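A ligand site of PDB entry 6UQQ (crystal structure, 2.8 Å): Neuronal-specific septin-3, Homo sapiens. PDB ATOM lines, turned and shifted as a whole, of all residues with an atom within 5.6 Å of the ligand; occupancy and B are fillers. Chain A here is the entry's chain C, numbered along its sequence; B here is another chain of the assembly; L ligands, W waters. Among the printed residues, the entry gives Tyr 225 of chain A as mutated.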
ATOM      1  N   GLN A  12      22.193   8.615 -19.012  1.00  0.00           N
ATOM      2  CA  GLN A  12      21.254   8.480 -17.913  1.00  0.00           C
ATOM      3  C   GLN A  12      19.849   8.252 -18.449  1.00  0.00           C
ATOM      4  O   GLN A  12      19.489   8.710 -19.535  1.00  0.00           O
ATOM      5  CB  GLN A  12      21.287   9.717 -17.019  1.00  0.00           C
ATOM      6  CG  GLN A  12      22.612   9.975 -16.335  1.00  0.00           C
ATOM      7  CD  GLN A  12      22.628  11.310 -15.612  1.00  0.00           C
ATOM      8  OE1 GLN A  12      21.707  12.110 -15.739  1.00  0.00           O
ATOM      9  NE2 GLN A  12      23.681  11.542 -14.839  1.00  0.00           N
ATOM     10  N   SER A  13      19.036   7.559 -17.667  1.00  0.00           N
ATOM     11  CA  SER A  13      17.665   7.274 -18.071  1.00  0.00           C
ATOM     12  C   SER A  13      16.852   8.553 -18.092  1.00  0.00           C
ATOM     13  O   SER A  13      16.843   9.315 -17.122  1.00  0.00           O
ATOM     14  CB  SER A  13      17.036   6.256 -17.119  1.00  0.00           C
ATOM     15  OG  SER A  13      15.678   6.023 -17.462  1.00  0.00           O
ATOM     16  N   GLY A  14      16.155   8.787 -19.206  1.00  0.00           N
ATOM     17  CA  GLY A  14      15.305   9.949 -19.338  1.00  0.00           C
ATOM     18  C   GLY A  14      15.986  11.117 -20.013  1.00  0.00           C
ATOM     19  O   GLY A  14      15.781  12.266 -19.629  1.00  0.00           O
ATOM     20  N   LEU A  15      16.808  10.826 -21.034  1.00  0.00           N
ATOM     21  CA  LEU A  15      17.481  11.848 -21.814  1.00  0.00           C
ATOM     22  C   LEU A  15      16.988  11.918 -23.245  1.00  0.00           C
ATOM     23  O   LEU A  15      17.538  12.678 -24.048  1.00  0.00           O
ATOM     24  CB  LEU A  15      18.995  11.613 -21.784  1.00  0.00           C
ATOM     25  CG  LEU A  15      19.735  11.959 -20.491  1.00  0.00           C
ATOM     26  CD1 LEU A  15      21.220  11.688 -20.628  1.00  0.00           C
ATOM     27  CD2 LEU A  15      19.499  13.404 -20.101  1.00  0.00           C
ATOM     28  N   GLY A  16      15.948  11.147 -23.585  1.00  0.00           N
ATOM     29  CA  GLY A  16      15.456  11.098 -24.944  1.00  0.00           C
ATOM     30  C   GLY A  16      16.194  10.116 -25.839  1.00  0.00           C
ATOM     31  O   GLY A  16      16.085  10.233 -27.059  1.00  0.00           O
ATOM     32  N   LYS A  17      16.920   9.151 -25.264  1.00  0.00           N
ATOM     33  CA  LYS A  17      17.750   8.259 -26.065  1.00  0.00           C
ATOM     34  C   LYS A  17      16.914   7.444 -27.049  1.00  0.00           C
ATOM     35  O   LYS A  17      17.157   7.482 -28.267  1.00  0.00           O
ATOM     36  CB  LYS A  17      18.563   7.340 -25.143  1.00  0.00           C
ATOM     37  CG  LYS A  17      19.647   8.048 -24.346  1.00  0.00           C
ATOM     38  CD  LYS A  17      20.243   7.124 -23.289  1.00  0.00           C
ATOM     39  CE  LYS A  17      19.143   6.489 -22.464  1.00  0.00           C
ATOM     40  NZ  LYS A  17      19.522   6.251 -21.042  1.00  0.00           N
ATOM     41  N   SER A  18      15.932   6.697 -26.550  1.00  0.00           N
ATOM     42  CA  SER A  18      15.108   5.880 -27.431  1.00  0.00           C
ATOM     43  C   SER A  18      14.225   6.726 -28.339  1.00  0.00           C
ATOM     44  O   SER A  18      13.849   6.260 -29.420  1.00  0.00           O
ATOM     45  CB  SER A  18      14.242   4.916 -26.609  1.00  0.00           C
ATOM     46  OG  SER A  18      13.354   5.623 -25.775  1.00  0.00           O
ATOM     47  N   THR A  19      13.874   7.947 -27.937  1.00  0.00           N
ATOM     48  CA  THR A  19      13.105   8.810 -28.819  1.00  0.00           C
ATOM     49  C   THR A  19      13.971   9.318 -29.965  1.00  0.00           C
ATOM     50  O   THR A  19      13.503   9.400 -31.114  1.00  0.00           O
ATOM     51  CB  THR A  19      12.499   9.986 -28.041  1.00  0.00           C
ATOM     52  OG1 THR A  19      11.546   9.497 -27.091  1.00  0.00           O
ATOM     53  CG2 THR A  19      11.795  10.966 -28.975  1.00  0.00           C
ATOM     54  N   LEU A  20      15.234   9.636 -29.688  1.00  0.00           N
ATOM     55  CA  LEU A  20      16.115  10.127 -30.739  1.00  0.00           C
ATOM     56  C   LEU A  20      16.399   9.035 -31.774  1.00  0.00           C
ATOM     57  O   LEU A  20      16.394   9.305 -32.981  1.00  0.00           O
ATOM     58  CB  LEU A  20      17.424  10.629 -30.150  1.00  0.00           C
ATOM     59  CG  LEU A  20      18.296  11.293 -31.213  1.00  0.00           C
ATOM     60  CD1 LEU A  20      17.774  12.691 -31.533  1.00  0.00           C
ATOM     61  CD2 LEU A  20      19.765  11.333 -30.826  1.00  0.00           C
ATOM     62  N   LYS A  32      11.830  -0.037 -26.922  1.00  0.00           N
ATOM     63  CA  LYS A  32      10.532   0.221 -26.287  1.00  0.00           C
ATOM     64  C   LYS A  32       9.506   0.576 -27.359  1.00  0.00           C
ATOM     65  O   LYS A  32       9.639   1.602 -28.023  1.00  0.00           O
ATOM     66  CB  LYS A  32      10.678   1.337 -25.271  1.00  0.00           C
ATOM     67  CG  LYS A  32      11.991   1.281 -24.509  1.00  0.00           C
ATOM     68  CD  LYS A  32      12.183   2.492 -23.602  1.00  0.00           C
ATOM     69  CE  LYS A  32      13.547   2.448 -22.925  1.00  0.00           C
ATOM     70  NZ  LYS A  32      13.954   3.803 -22.442  1.00  0.00           N
ATOM     71  N   ARG A  38       7.244   1.024 -22.746  1.00  0.00           N
ATOM     72  CA  ARG A  38       7.965   2.291 -22.758  1.00  0.00           C
ATOM     73  C   ARG A  38       8.263   2.762 -21.341  1.00  0.00           C
ATOM     74  O   ARG A  38       9.341   3.314 -21.075  1.00  0.00           O
ATOM     75  CB  ARG A  38       7.159   3.343 -23.521  1.00  0.00           C
ATOM     76  CG  ARG A  38       6.636   2.861 -24.862  1.00  0.00           C
ATOM     77  CD  ARG A  38       5.786   3.936 -25.527  1.00  0.00           C
ATOM     78  NE  ARG A  38       5.194   3.455 -26.777  1.00  0.00           N
ATOM     79  CZ  ARG A  38       5.825   3.459 -27.951  1.00  0.00           C
ATOM     80  NH1 ARG A  38       5.207   3.002 -29.032  1.00  0.00           N
ATOM     81  NH2 ARG A  38       7.064   3.926 -28.046  1.00  0.00           N
ATOM     82  N   LYS A 151      18.133  16.662 -25.151  1.00  0.00           N
ATOM     83  CA  LYS A 151      17.054  17.627 -24.930  1.00  0.00           C
ATOM     84  C   LYS A 151      17.523  19.056 -25.183  1.00  0.00           C
ATOM     85  O   LYS A 151      17.564  19.906 -24.280  1.00  0.00           O
ATOM     86  CB  LYS A 151      16.489  17.481 -23.517  1.00  0.00           C
ATOM     87  CG  LYS A 151      15.973  16.089 -23.159  1.00  0.00           C
ATOM     88  CD  LYS A 151      15.224  16.129 -21.828  1.00  0.00           C
ATOM     89  CE  LYS A 151      14.905  14.740 -21.300  1.00  0.00           C
ATOM     90  NZ  LYS A 151      13.938  13.983 -22.151  1.00  0.00           N
ATOM     91  N   ALA A 152      17.883  19.337 -26.436  1.00  0.00           N
ATOM     92  CA  ALA A 152      18.410  20.657 -26.760  1.00  0.00           C
ATOM     93  C   ALA A 152      17.353  21.745 -26.705  1.00  0.00           C
ATOM     94  O   ALA A 152      17.694  22.933 -26.699  1.00  0.00           O
ATOM     95  CB  ALA A 152      19.063  20.644 -28.146  1.00  0.00           C
ATOM     96  N   ASP A 153      16.069  21.370 -26.656  1.00  0.00           N
ATOM     97  CA  ASP A 153      15.001  22.358 -26.531  1.00  0.00           C
ATOM     98  C   ASP A 153      14.939  22.969 -25.137  1.00  0.00           C
ATOM     99  O   ASP A 153      14.158  23.898 -24.933  1.00  0.00           O
ATOM    100  CB  ASP A 153      13.652  21.731 -26.894  1.00  0.00           C
ATOM    101  CG  ASP A 153      13.472  20.347 -26.317  1.00  0.00           C
ATOM    102  OD1 ASP A 153      14.496  19.706 -26.016  1.00  0.00           O
ATOM    103  OD2 ASP A 153      12.318  19.892 -26.184  1.00  0.00           O
ATOM    104  N   THR A 154      15.743  22.479 -24.192  1.00  0.00           N
ATOM    105  CA  THR A 154      15.777  23.011 -22.835  1.00  0.00           C
ATOM    106  C   THR A 154      16.822  24.107 -22.656  1.00  0.00           C
ATOM    107  O   THR A 154      17.141  24.452 -21.522  1.00  0.00           O
ATOM    108  CB  THR A 154      16.039  21.881 -21.830  1.00  0.00           C
ATOM    109  OG1 THR A 154      17.430  21.577 -21.817  1.00  0.00           O
ATOM    110  CG2 THR A 154      15.248  20.646 -22.209  1.00  0.00           C
ATOM    111  N   VAL A 206      20.780  17.860 -29.973  1.00  0.00           N
ATOM    112  CA  VAL A 206      19.729  17.129 -30.655  1.00  0.00           C
ATOM    113  C   VAL A 206      18.403  17.280 -29.919  1.00  0.00           C
ATOM    114  O   VAL A 206      18.359  17.546 -28.707  1.00  0.00           O
ATOM    115  CB  VAL A 206      20.089  15.635 -30.825  1.00  0.00           C
ATOM    116  CG1 VAL A 206      21.406  15.489 -31.562  1.00  0.00           C
ATOM    117  CG2 VAL A 206      20.157  14.956 -29.473  1.00  0.00           C
ATOM    118  N   VAL A 207      17.321  17.120 -30.664  1.00  0.00           N
ATOM    119  CA  VAL A 207      15.968  17.023 -30.127  1.00  0.00           C
ATOM    120  C   VAL A 207      15.273  15.868 -30.847  1.00  0.00           C
ATOM    121  O   VAL A 207      15.320  15.777 -32.071  1.00  0.00           O
ATOM    122  CB  VAL A 207      15.162  18.326 -30.315  1.00  0.00           C
ATOM    123  CG1 VAL A 207      13.694  18.126 -29.952  1.00  0.00           C
ATOM    124  CG2 VAL A 207      15.769  19.450 -29.487  1.00  0.00           C
ATOM    125  N   GLY A 208      14.640  14.985 -30.082  1.00  0.00           N
ATOM    126  CA  GLY A 208      13.884  13.874 -30.637  1.00  0.00           C
ATOM    127  C   GLY A 208      12.390  14.099 -30.462  1.00  0.00           C
ATOM    128  O   GLY A 208      11.959  14.764 -29.521  1.00  0.00           O
ATOM    129  N   SER A 209      11.605  13.550 -31.382  1.00  0.00           N
ATOM    130  CA  SER A 209      10.153  13.640 -31.274  1.00  0.00           C
ATOM    131  C   SER A 209       9.516  12.527 -32.084  1.00  0.00           C
ATOM    132  O   SER A 209      10.006  12.150 -33.147  1.00  0.00           O
ATOM    133  CB  SER A 209       9.633  14.998 -31.739  1.00  0.00           C
ATOM    134  OG  SER A 209       8.215  15.021 -31.681  1.00  0.00           O
ATOM    135  N   ARG A 223       7.963  19.001 -30.864  1.00  0.00           N
ATOM    136  CA  ARG A 223       7.364  18.920 -29.544  1.00  0.00           C
ATOM    137  C   ARG A 223       6.489  20.141 -29.310  1.00  0.00           C
ATOM    138  O   ARG A 223       6.925  21.269 -29.559  1.00  0.00           O
ATOM    139  CB  ARG A 223       8.442  18.821 -28.468  1.00  0.00           C
ATOM    140  CG  ARG A 223       9.308  17.568 -28.574  1.00  0.00           C
ATOM    141  CD  ARG A 223      10.496  17.624 -27.639  1.00  0.00           C
ATOM    142  NE  ARG A 223      10.110  17.991 -26.279  1.00  0.00           N
ATOM    143  CZ  ARG A 223       9.535  17.161 -25.422  1.00  0.00           C
ATOM    144  NH1 ARG A 223       9.263  15.913 -25.773  1.00  0.00           N
ATOM    145  NH2 ARG A 223       9.226  17.573 -24.194  1.00  0.00           N
ATOM    146  N   TYR A 225       4.619  22.726 -27.080  1.00  0.00           N
ATOM    147  CA  TYR A 225       4.489  23.418 -25.801  1.00  0.00           C
ATOM    148  C   TYR A 225       3.349  24.427 -25.873  1.00  0.00           C
ATOM    149  O   TYR A 225       2.929  24.825 -26.968  1.00  0.00           O
ATOM    150  CB  TYR A 225       5.794  24.143 -25.446  1.00  0.00           C
ATOM    151  CG  TYR A 225       6.954  23.227 -25.127  1.00  0.00           C
ATOM    152  CD1 TYR A 225       7.020  22.561 -23.909  1.00  0.00           C
ATOM    153  CD2 TYR A 225       7.977  23.031 -26.045  1.00  0.00           C
ATOM    154  CE1 TYR A 225       8.080  21.728 -23.615  1.00  0.00           C
ATOM    155  CE2 TYR A 225       9.037  22.196 -25.761  1.00  0.00           C
ATOM    156  CZ  TYR A 225       9.086  21.541 -24.545  1.00  0.00           C
ATOM    157  OH  TYR A 225      10.137  20.711 -24.261  1.00  0.00           O
ATOM    158  N   SER B 135      12.989  13.934 -15.741  1.00  0.00           N
ATOM    159  CA  SER B 135      13.159  12.795 -16.644  1.00  0.00           C
ATOM    160  C   SER B 135      11.942  12.621 -17.537  1.00  0.00           C
ATOM    161  O   SER B 135      12.071  12.306 -18.721  1.00  0.00           O
ATOM    162  CB  SER B 135      13.373  11.515 -15.835  1.00  0.00           C
ATOM    163  OG  SER B 135      14.341  11.727 -14.814  1.00  0.00           O
ATOM    164  N   GLY B 136      10.753  12.830 -16.986  1.00  0.00           N
ATOM    165  CA  GLY B 136       9.531  12.387 -17.607  1.00  0.00           C
ATOM    166  C   GLY B 136       9.191  10.945 -17.302  1.00  0.00           C
ATOM    167  O   GLY B 136       8.174  10.453 -17.804  1.00  0.00           O
ATOM    168  N   HIS B 137      10.017  10.256 -16.514  1.00  0.00           N
ATOM    169  CA  HIS B 137       9.754   8.875 -16.139  1.00  0.00           C
ATOM    170  C   HIS B 137       9.198   8.820 -14.722  1.00  0.00           C
ATOM    171  O   HIS B 137       7.976   8.843 -14.513  1.00  0.00           O
ATOM    172  CB  HIS B 137      11.028   8.039 -16.222  1.00  0.00           C
ATOM    173  CG  HIS B 137      11.462   7.743 -17.626  1.00  0.00           C
ATOM    174  ND1 HIS B 137      10.813   6.841 -18.433  1.00  0.00           N
ATOM    175  CD2 HIS B 137      12.498   8.233 -18.353  1.00  0.00           C
ATOM    176  CE1 HIS B 137      11.420   6.788 -19.607  1.00  0.00           C
ATOM    177  NE2 HIS B 137      12.446   7.617 -19.583  1.00  0.00           N
ATOM    178  N   ASP B 164       9.754  23.593 -18.204  1.00  0.00           N
ATOM    179  CA  ASP B 164       9.710  23.795 -19.653  1.00  0.00           C
ATOM    180  C   ASP B 164      10.354  22.643 -20.426  1.00  0.00           C
ATOM    181  O   ASP B 164      10.249  22.612 -21.659  1.00  0.00           O
ATOM    182  CB  ASP B 164      10.394  25.116 -20.010  1.00  0.00           C
ATOM    183  CG  ASP B 164      11.683  25.330 -19.236  1.00  0.00           C
ATOM    184  OD1 ASP B 164      11.909  24.576 -18.268  1.00  0.00           O
ATOM    185  OD2 ASP B 164      12.446  26.241 -19.601  1.00  0.00           O
ATOM    186  N   THR B 165      11.014  21.706 -19.733  1.00  0.00           N
ATOM    187  CA  THR B 165      11.541  20.519 -20.387  1.00  0.00           C
ATOM    188  C   THR B 165      10.421  19.593 -20.870  1.00  0.00           C
ATOM    189  O   THR B 165      10.608  18.870 -21.859  1.00  0.00           O
ATOM    190  CB  THR B 165      12.469  19.776 -19.416  1.00  0.00           C
ATOM    191  OG1 THR B 165      13.562  20.633 -19.073  1.00  0.00           O
ATOM    192  CG2 THR B 165      13.009  18.482 -20.020  1.00  0.00           C
ATOM    193  N   LEU B 166       9.263  19.620 -20.225  1.00  0.00           N
ATOM    194  CA  LEU B 166       8.200  18.653 -20.478  1.00  0.00           C
ATOM    195  C   LEU B 166       6.993  19.323 -21.118  1.00  0.00           C
ATOM    196  O   LEU B 166       6.584  20.415 -20.702  1.00  0.00           O
ATOM    197  CB  LEU B 166       7.788  17.969 -19.182  1.00  0.00           C
ATOM    198  CG  LEU B 166       8.948  17.491 -18.313  1.00  0.00           C
ATOM    199  CD1 LEU B 166       8.739  17.928 -16.875  1.00  0.00           C
ATOM    200  CD2 LEU B 166       9.090  15.983 -18.396  1.00  0.00           C
ATOM    201  N   GLU B 170       3.409  15.142 -21.011  1.00  0.00           N
ATOM    202  CA  GLU B 170       4.493  14.453 -20.316  1.00  0.00           C
ATOM    203  C   GLU B 170       4.546  14.860 -18.856  1.00  0.00           C
ATOM    204  O   GLU B 170       4.651  14.012 -17.961  1.00  0.00           O
ATOM    205  CB  GLU B 170       5.829  14.749 -21.001  1.00  0.00           C
ATOM    206  CG  GLU B 170       5.925  14.299 -22.445  1.00  0.00           C
ATOM    207  CD  GLU B 170       7.064  14.973 -23.186  1.00  0.00           C
ATOM    208  OE1 GLU B 170       7.741  15.830 -22.585  1.00  0.00           O
ATOM    209  OE2 GLU B 170       7.282  14.648 -24.379  1.00  0.00           O
ATOM    210  N   GLN B 173       1.604  13.122 -16.575  1.00  0.00           N
ATOM    211  CA  GLN B 173       1.833  11.772 -16.099  1.00  0.00           C
ATOM    212  C   GLN B 173       3.129  11.635 -15.313  1.00  0.00           C
ATOM    213  O   GLN B 173       3.244  10.737 -14.470  1.00  0.00           O
ATOM    214  CB  GLN B 173       1.815  10.763 -17.258  1.00  0.00           C
ATOM    215  CG  GLN B 173       3.039  10.747 -18.139  1.00  0.00           C
ATOM    216  CD  GLN B 173       2.955   9.664 -19.213  1.00  0.00           C
ATOM    217  OE1 GLN B 173       1.925   9.019 -19.362  1.00  0.00           O
ATOM    218  NE2 GLN B 173       4.056   9.455 -19.936  1.00  0.00           N
HETATM  219  P1  LIG L   1      15.344   7.439 -22.705  1.00  0.00           P
HETATM  220  O1  LIG L   1      15.753   6.300 -23.631  1.00  0.00           O
HETATM  221  O2  LIG L   1      16.586   8.122 -22.209  1.00  0.00           O
HETATM  222  O3  LIG L   1      14.571   6.916 -21.517  1.00  0.00           O
HETATM  223  O4  LIG L   1      14.513   8.560 -23.501  1.00  0.00           O
HETATM  224  P2  LIG L   1      12.913   8.578 -23.643  1.00  0.00           P
HETATM  225  O5  LIG L   1      12.565   8.478 -25.106  1.00  0.00           O
HETATM  226  O6  LIG L   1      12.225   7.449 -22.904  1.00  0.00           O
HETATM  227  O7  LIG L   1      12.532  10.029 -23.069  1.00  0.00           O
HETATM  228  C1  LIG L   1      11.878  10.212 -21.806  1.00  0.00           C
HETATM  229  C2  LIG L   1      11.006  11.444 -21.890  1.00  0.00           C
HETATM  230  O8  LIG L   1      11.711  12.526 -22.498  1.00  0.00           O
HETATM  231  C3  LIG L   1       9.793  11.162 -22.773  1.00  0.00           C
HETATM  232  O9  LIG L   1       8.612  11.474 -22.027  1.00  0.00           O
HETATM  233  C4  LIG L   1       9.947  12.076 -23.967  1.00  0.00           C
HETATM  234  O10 LIG L   1       8.678  12.635 -24.321  1.00  0.00           O
HETATM  235  C5  LIG L   1      10.908  13.160 -23.500  1.00  0.00           C
HETATM  236  N1  LIG L   1      11.761  13.635 -24.610  1.00  0.00           N
HETATM  237  C6  LIG L   1      12.223  12.908 -25.651  1.00  0.00           C
HETATM  238  N2  LIG L   1      12.992  13.657 -26.474  1.00  0.00           N
HETATM  239  C7  LIG L   1      13.033  14.902 -25.958  1.00  0.00           C
HETATM  240  C8  LIG L   1      13.657  16.201 -26.320  1.00  0.00           C
HETATM  241  O11 LIG L   1      14.359  16.307 -27.351  1.00  0.00           O
HETATM  242  N3  LIG L   1      13.452  17.249 -25.512  1.00  0.00           N
HETATM  243  C9  LIG L   1      12.698  17.167 -24.403  1.00  0.00           C
HETATM  244  N4  LIG L   1      12.549  18.279 -23.638  1.00  0.00           N
HETATM  245  N5  LIG L   1      12.093  16.018 -24.007  1.00  0.00           N
HETATM  246  C10 LIG L   1      12.221  14.880 -24.727  1.00  0.00           C
HETATM  247  O   HOH W   1      15.619  12.794 -27.956  1.00  0.00           O
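Water W1 lies within hydrogen-bond range of O of Gly 16 (2.8 Å), N2 of the ligand (3.1 Å) and N of Gly 208 (3.2 Å).
OD2 of Asp 153 is in salt-bridge range of NE of Arg 223 (2.9 Å). The backbone carbonyl oxygen of Gln 12 is in hydrogen-bond range of the side-chain amino group of Lys 17, 2.9 Å away. The backbone carbonyl oxygen of Lys 151 lies within hydrogen-bond range of the side-chain hydroxyl of Thr 154 (3.0 Å). The backbone carbonyl oxygen (O) of Thr 165 of chain B is in hydrogen-bond range of the guanidinium group (NH2) of Arg 223, 3.0 Å away. OE2 of Glu 170 of chain B lies within salt-bridge range of NH1 of Arg 223 (2.7 Å). The backbone carbonyl oxygen of Lys 32 is in hydrogen-bond range of the guanidinium group of Arg 38, 3.5 Å away. The side-chain hydroxyl (OH) of Tyr 225 sits close to the backbone carbonyl oxygen (O) of Asp 164 of chain B (3.2 Å). The side-chain hydroxyl (OH) of Tyr 225 is in hydrogen-bond range of the backbone carbonyl oxygen (O) of Thr 165 of chain B.
An oxygen (O8) of the ligand lies within hydrogen-bond range of the side-chain amino group (NZ) of Lys 151 (2.7 Å). An oxygen (O4) of the ligand sits at hydrogen-bond distance from the backbone NH (N) of Lys 17 (3.0 Å). An oxygen (O1) of the ligand sits at hydrogen-bond distance from the backbone NH (N) of Ser 18, at 3.0 Å. OH of Tyr 225 is in hydrogen-bond range of N4 of the ligand (3.5 Å). A nitrogen (N4) of the ligand lies within hydrogen-bond range of the backbone carbonyl oxygen (O) of Thr 165 of chain B (2.7 Å). The side-chain amino group of Lys 17 lies within salt-bridge range of an oxygen (O2) of the ligand, 3.7 Å away. N5 of the ligand sits close to NH2 of Arg 223 (3.3 Å). N of Gly 208 sits at hydrogen-bond distance from O11 of the ligand, 3.0 Å away. The side-chain hydroxyl (OG) of Ser 18 sits at hydrogen-bond distance from an oxygen (O5) of the ligand, at 3.0 Å. O10 of the ligand lies within hydrogen-bond range of OE2 of Glu 170 of chain B (2.5 Å). An oxygen (O1) of the ligand is in salt-bridge range of the side-chain amino group (NZ) of Lys 32, at 3.3 Å. The backbone NH (N) of Thr 19 sits at hydrogen-bond distance from an oxygen (O5) of the ligand, 3.2 Å away. The side-chain carboxylate of Asp 153 is in hydrogen-bond range of a nitrogen (N3) of the ligand, at 2.7 Å. A ring nitrogen (NE2) of His 137 of chain B is in hydrogen-bond range of an oxygen (O3) of the ligand, 3.0 Å away. N of Gly 16 is in hydrogen-bond range of O4 of the ligand (3.0 Å). N of Leu 15 sits at hydrogen-bond distance from O2 of the ligand, at 3.0 Å. N of Gly 14 is in hydrogen-bond range of O2 of the ligand, at 3.1 Å. OG1 of Thr 19 lies within hydrogen-bond range of O5 of the ligand.
Gln 12 touches the ligand (O to O2, 3.99 Å). CG2 of Thr 154 touches N4 of the ligand, at 3.9 Å. Val 207 touches the ligand. Ser 135 of chain B touches the ligand (O to C2, 3.5 Å). 19 residues have an atom within 4 Å of the ligand: Gln 12, Gly 14, Leu 15, Gly 16, Lys 17, Ser 18, Thr 19, Lys 32, Lys 151, Asp 153, Thr 154, Val 207, Gly 208, Arg 223, Tyr 225, Ser 135 of chain B, His 137 of chain B, Thr 165 of chain B and Glu 170 of chain B. The nearest printed residue that does not touch the ligand is Ser 13 (4.1 Å).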
